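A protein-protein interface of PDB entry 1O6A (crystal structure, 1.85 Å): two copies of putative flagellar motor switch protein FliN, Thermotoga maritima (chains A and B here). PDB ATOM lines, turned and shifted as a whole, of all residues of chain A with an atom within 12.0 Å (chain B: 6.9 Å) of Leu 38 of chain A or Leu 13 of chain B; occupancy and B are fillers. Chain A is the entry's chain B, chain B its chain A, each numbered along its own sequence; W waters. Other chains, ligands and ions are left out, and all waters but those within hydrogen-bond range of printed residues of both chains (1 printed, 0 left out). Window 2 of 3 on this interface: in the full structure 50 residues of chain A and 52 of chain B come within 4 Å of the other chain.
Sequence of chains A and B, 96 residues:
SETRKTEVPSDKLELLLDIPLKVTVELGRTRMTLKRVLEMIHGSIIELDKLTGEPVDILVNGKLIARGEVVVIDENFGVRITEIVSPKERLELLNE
The backbone carbonyl oxygen (O) of Met 32 of chain A sits at hydrogen-bond distance from the backbone NH (N) of Leu 21 of chain B. The backbone NH (N) of Lys 35 of chain A sits at hydrogen-bond distance from the backbone carbonyl oxygen (O) of Leu 17 of chain B. The guanidinium group of Arg 90 of chain B is in hydrogen-bond range of the backbone carbonyl oxygen of Met 40 of chain A (2.8 Å). NH1 of Arg 90 of chain B sits at hydrogen-bond distance from O of Leu 38 of chain A, 3.3 Å away. O of Leu 17 of chain B sits close to OG1 of Thr 33 of chain A (3.4 Å). The backbone carbonyl oxygen of Val 37 of chain A sits at hydrogen-bond distance from the guanidinium group of Arg 90 of chain B.
No position is printed for both chains.
Hydrophobic or aromatic side chains of chain B that line the printed part of chain A: Leu 13, Leu 16, Leu 21, Ile 65, Pro 87 and Leu 94. Of the 16 printed residues of chain A, 8 touch a printed residue of chain B. Among the printed residues, no Asp or Glu carboxylate lies within 4 Å of a Lys or Arg side-chain nitrogen of the other chain.
Among the printed residues, merely in contact across the chains: Arg 31 of chain A with Leu 21 of chain B (3.1 Å), Leu 34 of chain A with Leu 16 of chain B (3.4 Å), Thr 33 of chain A with Asp 18 of chain B (3.6 Å), Leu 38 of chain A with Pro 87 of chain B (3.6 Å), Leu 34 of chain A with Leu 17 of chain B (3.6 Å), Leu 34 of chain A with Leu 21 of chain B (3.8 Å), Met 40 of chain A with Ile 65 of chain B (3.8 Å), Val 37 of chain A with Leu 21 of chain B (3.8 Å), Leu 38 of chain A with Leu 13 of chain B (3.9 Å), Val 37 of chain A with Ile 65 of chain B (3.9 Å), Leu 34 of chain A with Leu 13 of chain B (3.9 Å) and Leu 34 of chain A with Leu 94 of chain B (3.9 Å).
Water W1 lies within hydrogen-bond range of the backbone carbonyl oxygen (O) of Leu 17 of chain B (2.9 Å), the side-chain carboxylate (OD1) of Asp 18 of chain B (2.9 Å) and the side-chain hydroxyl (OG1) of Thr 33 of chain A (3.3 Å).
Printed residues of chain B within 4 Å of Arg 31 of chain A: Leu 21. Of the printed residues of chain B, Thr 33 of chain A touches Leu 17 (3.2 Å) and Asp 18 (3.6 Å). Of the printed residues of chain B, Lys 35 of chain A touches Leu 17 (3.0 Å). Arg 36 of chain A touches none of the printed residues of chain B. Of the printed residues of chain B, Val 37 of chain A touches Leu 21 (3.8 Å), Ile 65 (3.9 Å) and Arg 90 (2.8 Å). Of chain B, only Leu 13 (3.9 Å), Pro 87 (3.6 Å) and Arg 90 (3.3 Å) come within 4 Å of Leu 38 of chain A. Ile 46 of chain A touches none of the printed residues of chain B. No residue of chain A comes within 4 Å of Ser 10 of chain B. No residue of chain A comes within 4 Å of Asp 11 of chain B. Leu 13 of chain B touches just these residues of chain A: Leu 34 and Leu 38. No residue of chain A comes within 4 Å of Glu 14 of chain B. Leu 15 of chain B touches none of the printed residues of chain A. Of chain A, only Leu 34 comes within 4 Å of Leu 16 of chain B. Printed residues of chain A within 4 Å of Leu 17 of chain B: Thr 33, Leu 34 and Lys 35. No residue of chain A comes within 4 Å of Leu 91 of chain B. The nearest residue of chain A that does not touch Leu 13 of chain B is Lys 35 of chain A (6.8 Å).
N of Arg 36 of chain A sits at hydrogen-bond distance from OG1 of Thr 33 of chain A, at 3.2 Å. N of Lys 35 of chain A lies close to OG1 of Thr 33 of chain A. NZ of Lys 35 of chain A is in salt-bridge range of OE1 of Glu 39 of chain A, at 3.3 Å.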
ATOM      1  N   ARG A  31     -24.818   7.404  16.801  1.00  0.00           N
ATOM      2  CA  ARG A  31     -23.391   7.340  17.029  1.00  0.00           C
ATOM      3  C   ARG A  31     -22.802   8.548  16.378  1.00  0.00           C
ATOM      4  O   ARG A  31     -23.241   8.995  15.307  1.00  0.00           O
ATOM      5  CB  ARG A  31     -22.788   6.049  16.448  1.00  0.00           C
ATOM      6  CG  ARG A  31     -23.398   4.759  16.980  1.00  0.00           C
ATOM      7  CD  ARG A  31     -22.778   3.489  16.400  1.00  0.00           C
ATOM      8  NE  ARG A  31     -22.710   3.639  14.961  1.00  0.00           N
ATOM      9  CZ  ARG A  31     -21.613   3.568  14.249  1.00  0.00           C
ATOM     10  NH1 ARG A  31     -20.477   3.177  14.819  1.00  0.00           N
ATOM     11  NH2 ARG A  31     -21.684   3.797  12.944  1.00  0.00           N
ATOM     12  N   MET A  32     -21.792   9.084  17.010  1.00  0.00           N
ATOM     13  CA  MET A  32     -21.031  10.166  16.423  1.00  0.00           C
ATOM     14  C   MET A  32     -19.586  10.077  16.881  1.00  0.00           C
ATOM     15  O   MET A  32     -19.286   9.384  17.849  1.00  0.00           O
ATOM     16  CB  MET A  32     -21.609  11.511  16.854  1.00  0.00           C
ATOM     17  CG  MET A  32     -21.629  11.680  18.289  1.00  0.00           C
ATOM     18  SD  MET A  32     -22.382  13.526  18.752  1.00  0.00           S
ATOM     19  CE  MET A  32     -23.925  13.400  18.019  1.00  0.00           C
ATOM     20  N   THR A  33     -18.706  10.785  16.209  1.00  0.00           N
ATOM     21  CA  THR A  33     -17.277  10.736  16.578  1.00  0.00           C
ATOM     22  C   THR A  33     -17.031  11.585  17.820  1.00  0.00           C
ATOM     23  O   THR A  33     -17.799  12.506  18.162  1.00  0.00           O
ATOM     24  CB  THR A  33     -16.328  11.200  15.461  1.00  0.00           C
ATOM     25  OG1 THR A  33     -16.509  12.602  15.216  1.00  0.00           O
ATOM     26  CG2 THR A  33     -16.552  10.442  14.125  1.00  0.00           C
ATOM     27  N   LEU A  34     -15.939  11.299  18.494  1.00  0.00           N
ATOM     28  CA  LEU A  34     -15.490  12.168  19.570  1.00  0.00           C
ATOM     29  C   LEU A  34     -15.318  13.626  19.115  1.00  0.00           C
ATOM     30  O   LEU A  34     -15.601  14.568  19.854  1.00  0.00           O
ATOM     31  CB  LEU A  34     -14.122  11.662  20.076  1.00  0.00           C
ATOM     32  CG  LEU A  34     -13.498  12.502  21.210  1.00  0.00           C
ATOM     33  CD1 LEU A  34     -14.367  12.519  22.437  1.00  0.00           C
ATOM     34  CD2 LEU A  34     -12.135  11.966  21.555  1.00  0.00           C
ATOM     35  N   LYS A  35     -14.816  13.839  17.910  1.00  0.00           N
ATOM     36  CA  LYS A  35     -14.650  15.197  17.408  1.00  0.00           C
ATOM     37  C   LYS A  35     -15.983  15.935  17.487  1.00  0.00           C
ATOM     38  O   LYS A  35     -16.074  17.025  18.052  1.00  0.00           O
ATOM     39  CB  LYS A  35     -14.159  15.193  15.965  1.00  0.00           C
ATOM     40  CG  LYS A  35     -13.778  16.586  15.438  1.00  0.00           C
ATOM     41  CD  LYS A  35     -13.271  16.496  13.987  1.00  0.00           C
ATOM     42  CE  LYS A  35     -13.787  17.628  13.091  1.00  0.00           C
ATOM     43  NZ  LYS A  35     -15.236  17.491  12.702  1.00  0.00           N
ATOM     44  N   ARG A  36     -17.017  15.284  16.974  1.00  0.00           N
ATOM     45  CA  ARG A  36     -18.340  15.885  16.936  1.00  0.00           C
ATOM     46  C   ARG A  36     -18.869  16.175  18.323  1.00  0.00           C
ATOM     47  O   ARG A  36     -19.466  17.237  18.568  1.00  0.00           O
ATOM     48  CB  ARG A  36     -19.315  15.014  16.149  1.00  0.00           C
ATOM     49  CG  ARG A  36     -20.636  15.713  15.967  1.00  0.00           C
ATOM     50  CD  ARG A  36     -21.653  15.017  15.118  1.00  0.00           C
ATOM     51  NE  ARG A  36     -22.977  15.568  15.403  1.00  0.00           N
ATOM     52  CZ  ARG A  36     -24.048  15.382  14.663  1.00  0.00           C
ATOM     53  NH1 ARG A  36     -24.002  14.626  13.564  1.00  0.00           N
ATOM     54  NH2 ARG A  36     -25.185  15.960  15.035  1.00  0.00           N
ATOM     55  N   VAL A  37     -18.674  15.233  19.233  1.00  0.00           N
ATOM     56  CA  VAL A  37     -19.117  15.389  20.610  1.00  0.00           C
ATOM     57  C   VAL A  37     -18.473  16.619  21.229  1.00  0.00           C
ATOM     58  O   VAL A  37     -19.155  17.394  21.927  1.00  0.00           O
ATOM     59  CB  VAL A  37     -18.821  14.116  21.462  1.00  0.00           C
ATOM     60  CG1 VAL A  37     -19.031  14.372  22.978  1.00  0.00           C
ATOM     61  CG2 VAL A  37     -19.701  12.986  21.008  1.00  0.00           C
ATOM     62  N   LEU A  38     -17.182  16.812  20.960  1.00  0.00           N
ATOM     63  CA  LEU A  38     -16.431  17.936  21.495  1.00  0.00           C
ATOM     64  C   LEU A  38     -16.743  19.294  20.832  1.00  0.00           C
ATOM     65  O   LEU A  38     -16.482  20.337  21.422  1.00  0.00           O
ATOM     66  CB  LEU A  38     -14.921  17.680  21.412  1.00  0.00           C
ATOM     67  CG  LEU A  38     -14.360  16.489  22.165  1.00  0.00           C
ATOM     68  CD1 LEU A  38     -12.865  16.425  21.949  1.00  0.00           C
ATOM     69  CD2 LEU A  38     -14.712  16.568  23.647  1.00  0.00           C
ATOM     70  N   GLU A  39     -17.294  19.277  19.628  1.00  0.00           N
ATOM     71  CA  GLU A  39     -17.685  20.498  18.905  1.00  0.00           C
ATOM     72  C   GLU A  39     -19.098  20.939  19.168  1.00  0.00           C
ATOM     73  O   GLU A  39     -19.473  22.069  18.796  1.00  0.00           O
ATOM     74  CB  GLU A  39     -17.535  20.272  17.398  1.00  0.00           C
ATOM     75  CG  GLU A  39     -16.073  20.227  16.986  1.00  0.00           C
ATOM     76  CD  GLU A  39     -15.853  19.984  15.489  1.00  0.00           C
ATOM     77  OE1 GLU A  39     -16.773  19.544  14.755  1.00  0.00           O
ATOM     78  OE2 GLU A  39     -14.732  20.241  15.059  1.00  0.00           O
ATOM     79  N   MET A  40     -19.913  20.073  19.769  1.00  0.00           N
ATOM     80  CA  MET A  40     -21.284  20.456  20.021  1.00  0.00           C
ATOM     81  C   MET A  40     -21.345  21.666  20.961  1.00  0.00           C
ATOM     82  O   MET A  40     -20.497  21.862  21.839  1.00  0.00           O
ATOM     83  CB  MET A  40     -22.101  19.297  20.595  1.00  0.00           C
ATOM     84  CG  MET A  40     -22.202  18.158  19.670  1.00  0.00           C
ATOM     85  SD  MET A  40     -23.567  16.951  20.355  1.00  0.00           S
ATOM     86  CE  MET A  40     -22.772  16.377  22.066  1.00  0.00           C
ATOM     87  N   ILE A  41     -22.340  22.508  20.713  1.00  0.00           N
ATOM     88  CA  ILE A  41     -22.617  23.694  21.514  1.00  0.00           C
ATOM     89  C   ILE A  41     -24.117  23.850  21.704  1.00  0.00           C
ATOM     90  O   ILE A  41     -24.904  23.083  21.153  1.00  0.00           O
ATOM     91  CB  ILE A  41     -22.033  24.933  20.832  1.00  0.00           C
ATOM     92  CG1 ILE A  41     -22.585  25.097  19.397  1.00  0.00           C
ATOM     93  CG2 ILE A  41     -20.497  24.862  20.813  1.00  0.00           C
ATOM     94  CD1 ILE A  41     -22.232  26.437  18.787  1.00  0.00           C
ATOM     95  N   HIS A  42     -24.503  24.815  22.525  1.00  0.00           N
ATOM     96  CA  HIS A  42     -25.921  25.203  22.668  1.00  0.00           C
ATOM     97  C   HIS A  42     -26.489  25.462  21.277  1.00  0.00           C
ATOM     98  O   HIS A  42     -25.908  26.212  20.503  1.00  0.00           O
ATOM     99  CB  HIS A  42     -26.070  26.435  23.572  1.00  0.00           C
ATOM    100  CG  HIS A  42     -25.621  26.201  24.992  1.00  0.00           C
ATOM    101  ND1 HIS A  42     -24.301  26.311  25.384  1.00  0.00           N
ATOM    102  CD2 HIS A  42     -26.304  25.828  26.099  1.00  0.00           C
ATOM    103  CE1 HIS A  42     -24.194  26.022  26.669  1.00  0.00           C
ATOM    104  NE2 HIS A  42     -25.400  25.742  27.130  1.00  0.00           N
ATOM    105  N   GLY A  43     -27.581  24.800  20.939  1.00  0.00           N
ATOM    106  CA  GLY A  43     -28.222  24.942  19.644  1.00  0.00           C
ATOM    107  C   GLY A  43     -27.843  23.856  18.640  1.00  0.00           C
ATOM    108  O   GLY A  43     -28.524  23.687  17.635  1.00  0.00           O
ATOM    109  N   SER A  44     -26.777  23.106  18.893  1.00  0.00           N
ATOM    110  CA  SER A  44     -26.454  21.955  18.035  1.00  0.00           C
ATOM    111  C   SER A  44     -27.639  20.961  18.022  1.00  0.00           C
ATOM    112  O   SER A  44     -28.373  20.832  18.981  1.00  0.00           O
ATOM    113  CB  SER A  44     -25.218  21.213  18.541  1.00  0.00           C
ATOM    114  OG  SER A  44     -24.041  21.947  18.374  1.00  0.00           O
ATOM    115  N   ILE A  45     -27.805  20.234  16.929  1.00  0.00           N
ATOM    116  CA  ILE A  45     -28.892  19.287  16.825  1.00  0.00           C
ATOM    117  C   ILE A  45     -28.315  17.892  16.631  1.00  0.00           C
ATOM    118  O   ILE A  45     -27.420  17.706  15.830  1.00  0.00           O
ATOM    119  CB  ILE A  45     -29.787  19.669  15.665  1.00  0.00           C
ATOM    120  CG1 ILE A  45     -30.674  20.851  16.083  1.00  0.00           C
ATOM    121  CG2 ILE A  45     -30.657  18.476  15.286  1.00  0.00           C
ATOM    122  CD1 ILE A  45     -31.327  21.525  14.962  1.00  0.00           C
ATOM    123  N   ILE A  46     -28.858  16.913  17.340  1.00  0.00           N
ATOM    124  CA  ILE A  46     -28.425  15.543  17.217  1.00  0.00           C
ATOM    125  C   ILE A  46     -29.618  14.782  16.644  1.00  0.00           C
ATOM    126  O   ILE A  46     -30.677  14.787  17.226  1.00  0.00           O
ATOM    127  CB  ILE A  46     -28.056  14.983  18.597  1.00  0.00           C
ATOM    128  CG1 ILE A  46     -26.881  15.771  19.215  1.00  0.00           C
ATOM    129  CG2 ILE A  46     -27.727  13.485  18.477  1.00  0.00           C
ATOM    130  CD1 ILE A  46     -26.518  15.262  20.626  1.00  0.00           C
ATOM    131  N   SER B  10      -3.419  15.789  23.850  1.00  0.00           N
ATOM    132  CA  SER B  10      -3.585  16.796  22.750  1.00  0.00           C
ATOM    133  C   SER B  10      -3.088  16.238  21.402  1.00  0.00           C
ATOM    134  O   SER B  10      -3.848  16.198  20.428  1.00  0.00           O
ATOM    135  CB  SER B  10      -2.871  18.102  23.108  1.00  0.00           C
ATOM    136  OG  SER B  10      -1.475  18.033  22.842  1.00  0.00           O
ATOM    137  N   ASP B  11      -1.819  15.815  21.346  1.00  0.00           N
ATOM    138  CA  ASP B  11      -1.370  14.931  20.268  1.00  0.00           C
ATOM    139  C   ASP B  11      -2.106  13.622  20.470  1.00  0.00           C
ATOM    140  O   ASP B  11      -2.543  12.989  19.506  1.00  0.00           O
ATOM    141  CB  ASP B  11       0.144  14.683  20.302  1.00  0.00           C
ATOM    142  CG  ASP B  11       0.939  15.745  19.546  1.00  0.00           C
ATOM    143  OD1 ASP B  11       0.351  16.460  18.695  1.00  0.00           O
ATOM    144  OD2 ASP B  11       2.168  15.926  19.742  1.00  0.00           O
ATOM    145  N   LYS B  12      -2.253  13.235  21.739  1.00  0.00           N
ATOM    146  CA  LYS B  12      -3.092  12.105  22.110  1.00  0.00           C
ATOM    147  C   LYS B  12      -4.526  12.311  21.588  1.00  0.00           C
ATOM    148  O   LYS B  12      -5.089  11.423  20.970  1.00  0.00           O
ATOM    149  CB  LYS B  12      -3.088  11.916  23.634  1.00  0.00           C
ATOM    150  CG  LYS B  12      -3.493  10.509  24.101  1.00  0.00           C
ATOM    151  CD  LYS B  12      -3.032  10.222  25.555  1.00  0.00           C
ATOM    152  CE  LYS B  12      -3.378   8.789  26.007  1.00  0.00           C
ATOM    153  NZ  LYS B  12      -4.725   8.312  25.508  1.00  0.00           N
ATOM    154  N   LEU B  13      -5.101  13.487  21.822  1.00  0.00           N
ATOM    155  CA  LEU B  13      -6.467  13.759  21.371  1.00  0.00           C
ATOM    156  C   LEU B  13      -6.628  13.542  19.850  1.00  0.00           C
ATOM    157  O   LEU B  13      -7.642  13.025  19.405  1.00  0.00           O
ATOM    158  CB  LEU B  13      -6.895  15.187  21.748  1.00  0.00           C
ATOM    159  CG  LEU B  13      -8.307  15.621  21.314  1.00  0.00           C
ATOM    160  CD1 LEU B  13      -9.353  14.734  21.916  1.00  0.00           C
ATOM    161  CD2 LEU B  13      -8.589  17.097  21.699  1.00  0.00           C
ATOM    162  N   GLU B  14      -5.636  13.959  19.067  1.00  0.00           N
ATOM    163  CA  GLU B  14      -5.701  13.881  17.603  1.00  0.00           C
ATOM    164  C   GLU B  14      -6.009  12.449  17.100  1.00  0.00           C
ATOM    165  O   GLU B  14      -6.760  12.243  16.118  1.00  0.00           O
ATOM    166  CB  GLU B  14      -4.383  14.409  17.020  1.00  0.00           C
ATOM    167  CG  GLU B  14      -4.260  14.436  15.503  1.00  0.00           C
ATOM    168  CD  GLU B  14      -5.311  15.289  14.806  1.00  0.00           C
ATOM    169  OE1 GLU B  14      -5.603  16.440  15.234  1.00  0.00           O
ATOM    170  OE2 GLU B  14      -5.858  14.789  13.809  1.00  0.00           O
ATOM    171  N   LEU B  15      -5.448  11.466  17.799  1.00  0.00           N
ATOM    172  CA  LEU B  15      -5.667  10.056  17.501  1.00  0.00           C
ATOM    173  C   LEU B  15      -7.059   9.552  17.848  1.00  0.00           C
ATOM    174  O   LEU B  15      -7.462   8.503  17.378  1.00  0.00           O
ATOM    175  CB  LEU B  15      -4.662   9.209  18.268  1.00  0.00           C
ATOM    176  CG  LEU B  15      -3.194   9.514  17.990  1.00  0.00           C
ATOM    177  CD1 LEU B  15      -2.337   8.537  18.791  1.00  0.00           C
ATOM    178  CD2 LEU B  15      -2.848   9.465  16.486  1.00  0.00           C
ATOM    179  N   LEU B  16      -7.789  10.291  18.677  1.00  0.00           N
ATOM    180  CA  LEU B  16      -9.087   9.851  19.177  1.00  0.00           C
ATOM    181  C   LEU B  16     -10.276  10.468  18.446  1.00  0.00           C
ATOM    182  O   LEU B  16     -11.418  10.097  18.697  1.00  0.00           O
ATOM    183  CB  LEU B  16      -9.210  10.230  20.660  1.00  0.00           C
ATOM    184  CG  LEU B  16      -8.100   9.701  21.564  1.00  0.00           C
ATOM    185  CD1 LEU B  16      -8.264  10.250  22.992  1.00  0.00           C
ATOM    186  CD2 LEU B  16      -8.146   8.211  21.553  1.00  0.00           C
ATOM    187  N   LEU B  17     -10.019  11.408  17.557  1.00  0.00           N
ATOM    188  CA  LEU B  17     -11.102  12.243  17.045  1.00  0.00           C
ATOM    189  C   LEU B  17     -12.127  11.489  16.237  1.00  0.00           C
ATOM    190  O   LEU B  17     -13.271  11.945  16.119  1.00  0.00           O
ATOM    191  CB  LEU B  17     -10.566  13.405  16.214  1.00  0.00           C
ATOM    192  CG  LEU B  17      -9.806  14.475  16.995  1.00  0.00           C
ATOM    193  CD1 LEU B  17      -9.289  15.504  16.005  1.00  0.00           C
ATOM    194  CD2 LEU B  17     -10.677  15.116  18.034  1.00  0.00           C
ATOM    195  N   ASP B  18     -11.723  10.368  15.650  1.00  0.00           N
ATOM    196  CA  ASP B  18     -12.612   9.593  14.778  1.00  0.00           C
ATOM    197  C   ASP B  18     -13.285   8.412  15.474  1.00  0.00           C
ATOM    198  O   ASP B  18     -14.018   7.683  14.849  1.00  0.00           O
ATOM    199  CB  ASP B  18     -11.841   9.104  13.528  1.00  0.00           C
ATOM    200  CG  ASP B  18     -12.385   9.699  12.226  1.00  0.00           C
ATOM    201  OD1 ASP B  18     -13.495  10.312  12.241  1.00  0.00           O
ATOM    202  OD2 ASP B  18     -11.745   9.621  11.154  1.00  0.00           O
ATOM    203  N   LEU B  21     -18.798   7.044  19.147  1.00  0.00           N
ATOM    204  CA  LEU B  21     -19.301   7.054  20.488  1.00  0.00           C
ATOM    205  C   LEU B  21     -20.783   6.849  20.411  1.00  0.00           C
ATOM    206  O   LEU B  21     -21.444   7.314  19.470  1.00  0.00           O
ATOM    207  CB  LEU B  21     -19.001   8.396  21.157  1.00  0.00           C
ATOM    208  CG  LEU B  21     -17.522   8.729  21.367  1.00  0.00           C
ATOM    209  CD1 LEU B  21     -17.415  10.074  22.024  1.00  0.00           C
ATOM    210  CD2 LEU B  21     -16.905   7.692  22.217  1.00  0.00           C
ATOM    211  N   ILE B  65     -23.706  14.293  29.469  1.00  0.00           N
ATOM    212  CA  ILE B  65     -22.903  15.476  29.112  1.00  0.00           C
ATOM    213  C   ILE B  65     -23.743  16.677  28.705  1.00  0.00           C
ATOM    214  O   ILE B  65     -23.229  17.794  28.616  1.00  0.00           O
ATOM    215  CB  ILE B  65     -21.885  15.178  28.027  1.00  0.00           C
ATOM    216  CG1 ILE B  65     -22.547  14.769  26.746  1.00  0.00           C
ATOM    217  CG2 ILE B  65     -20.835  14.101  28.448  1.00  0.00           C
ATOM    218  CD1 ILE B  65     -21.817  15.343  25.575  1.00  0.00           C
ATOM    219  N   SER B  86     -18.573  21.833  29.432  1.00  0.00           N
ATOM    220  CA  SER B  86     -17.470  22.312  28.584  1.00  0.00           C
ATOM    221  C   SER B  86     -16.808  21.146  27.831  1.00  0.00           C
ATOM    222  O   SER B  86     -16.871  19.991  28.282  1.00  0.00           O
ATOM    223  CB  SER B  86     -16.417  23.042  29.406  1.00  0.00           C
ATOM    224  OG  SER B  86     -15.676  22.111  30.179  1.00  0.00           O
ATOM    225  N   PRO B  87     -16.184  21.428  26.680  1.00  0.00           N
ATOM    226  CA  PRO B  87     -15.476  20.377  25.943  1.00  0.00           C
ATOM    227  C   PRO B  87     -14.426  19.664  26.795  1.00  0.00           C
ATOM    228  O   PRO B  87     -14.299  18.468  26.673  1.00  0.00           O
ATOM    229  CB  PRO B  87     -14.842  21.130  24.758  1.00  0.00           C
ATOM    230  CG  PRO B  87     -15.708  22.326  24.591  1.00  0.00           C
ATOM    231  CD  PRO B  87     -16.090  22.726  25.975  1.00  0.00           C
ATOM    232  N   LYS B  88     -13.728  20.377  27.659  1.00  0.00           N
ATOM    233  CA  LYS B  88     -12.804  19.757  28.596  1.00  0.00           C
ATOM    234  C   LYS B  88     -13.520  18.805  29.558  1.00  0.00           C
ATOM    235  O   LYS B  88     -13.037  17.705  29.814  1.00  0.00           O
ATOM    236  CB  LYS B  88     -12.082  20.831  29.396  1.00  0.00           C
ATOM    237  CG  LYS B  88     -10.951  20.286  30.244  1.00  0.00           C
ATOM    238  CD  LYS B  88     -10.080  21.413  30.812  1.00  0.00           C
ATOM    239  CE  LYS B  88      -9.588  21.089  32.233  1.00  0.00           C
ATOM    240  NZ  LYS B  88     -10.536  21.579  33.277  1.00  0.00           N
ATOM    241  N   GLU B  89     -14.683  19.207  30.080  1.00  0.00           N
ATOM    242  CA  GLU B  89     -15.437  18.323  30.983  1.00  0.00           C
ATOM    243  C   GLU B  89     -15.977  17.092  30.269  1.00  0.00           C
ATOM    244  O   GLU B  89     -16.101  16.025  30.873  1.00  0.00           O
ATOM    245  CB  GLU B  89     -16.557  19.082  31.687  1.00  0.00           C
ATOM    246  CG  GLU B  89     -16.022  20.148  32.653  1.00  0.00           C
ATOM    247  CD  GLU B  89     -17.092  21.092  33.214  1.00  0.00           C
ATOM    248  OE1 GLU B  89     -18.062  21.476  32.504  1.00  0.00           O
ATOM    249  OE2 GLU B  89     -16.946  21.492  34.389  1.00  0.00           O
ATOM    250  N   ARG B  90     -16.272  17.212  28.976  1.00  0.00           N
ATOM    251  CA  ARG B  90     -16.779  16.067  28.216  1.00  0.00           C
ATOM    252  C   ARG B  90     -15.660  15.003  28.121  1.00  0.00           C
ATOM    253  O   ARG B  90     -15.897  13.807  28.284  1.00  0.00           O
ATOM    254  CB  ARG B  90     -17.201  16.494  26.800  1.00  0.00           C
ATOM    255  CG  ARG B  90     -18.406  17.387  26.718  1.00  0.00           C
ATOM    256  CD  ARG B  90     -18.647  18.009  25.356  1.00  0.00           C
ATOM    257  NE  ARG B  90     -18.924  19.434  25.490  1.00  0.00           N
ATOM    258  CZ  ARG B  90     -19.204  20.253  24.494  1.00  0.00           C
ATOM    259  NH1 ARG B  90     -19.228  19.829  23.228  1.00  0.00           N
ATOM    260  NH2 ARG B  90     -19.454  21.530  24.777  1.00  0.00           N
ATOM    261  N   LEU B  91     -14.444  15.455  27.858  1.00  0.00           N
ATOM    262  CA  LEU B  91     -13.290  14.558  27.838  1.00  0.00           C
ATOM    263  C   LEU B  91     -13.067  13.865  29.160  1.00  0.00           C
ATOM    264  O   LEU B  91     -12.758  12.667  29.191  1.00  0.00           O
ATOM    265  CB  LEU B  91     -12.024  15.335  27.490  1.00  0.00           C
ATOM    266  CG  LEU B  91     -11.637  15.292  26.031  1.00  0.00           C
ATOM    267  CD1 LEU B  91     -10.340  16.083  25.855  1.00  0.00           C
ATOM    268  CD2 LEU B  91     -11.481  13.823  25.535  1.00  0.00           C
ATOM    269  N   LEU B  94     -15.728  11.192  29.849  1.00  0.00           N
ATOM    270  CA  LEU B  94     -15.573  10.048  28.960  1.00  0.00           C
ATOM    271  C   LEU B  94     -14.338   9.248  29.330  1.00  0.00           C
ATOM    272  O   LEU B  94     -14.248   8.075  28.992  1.00  0.00           O
ATOM    273  CB  LEU B  94     -15.466  10.496  27.498  1.00  0.00           C
ATOM    274  CG  LEU B  94     -16.774  11.045  26.954  1.00  0.00           C
ATOM    275  CD1 LEU B  94     -16.559  11.688  25.607  1.00  0.00           C
ATOM    276  CD2 LEU B  94     -17.817   9.937  26.890  1.00  0.00           C
HETATM  277  O   HOH W   1     -13.742  12.971  13.450  1.00  0.00           O
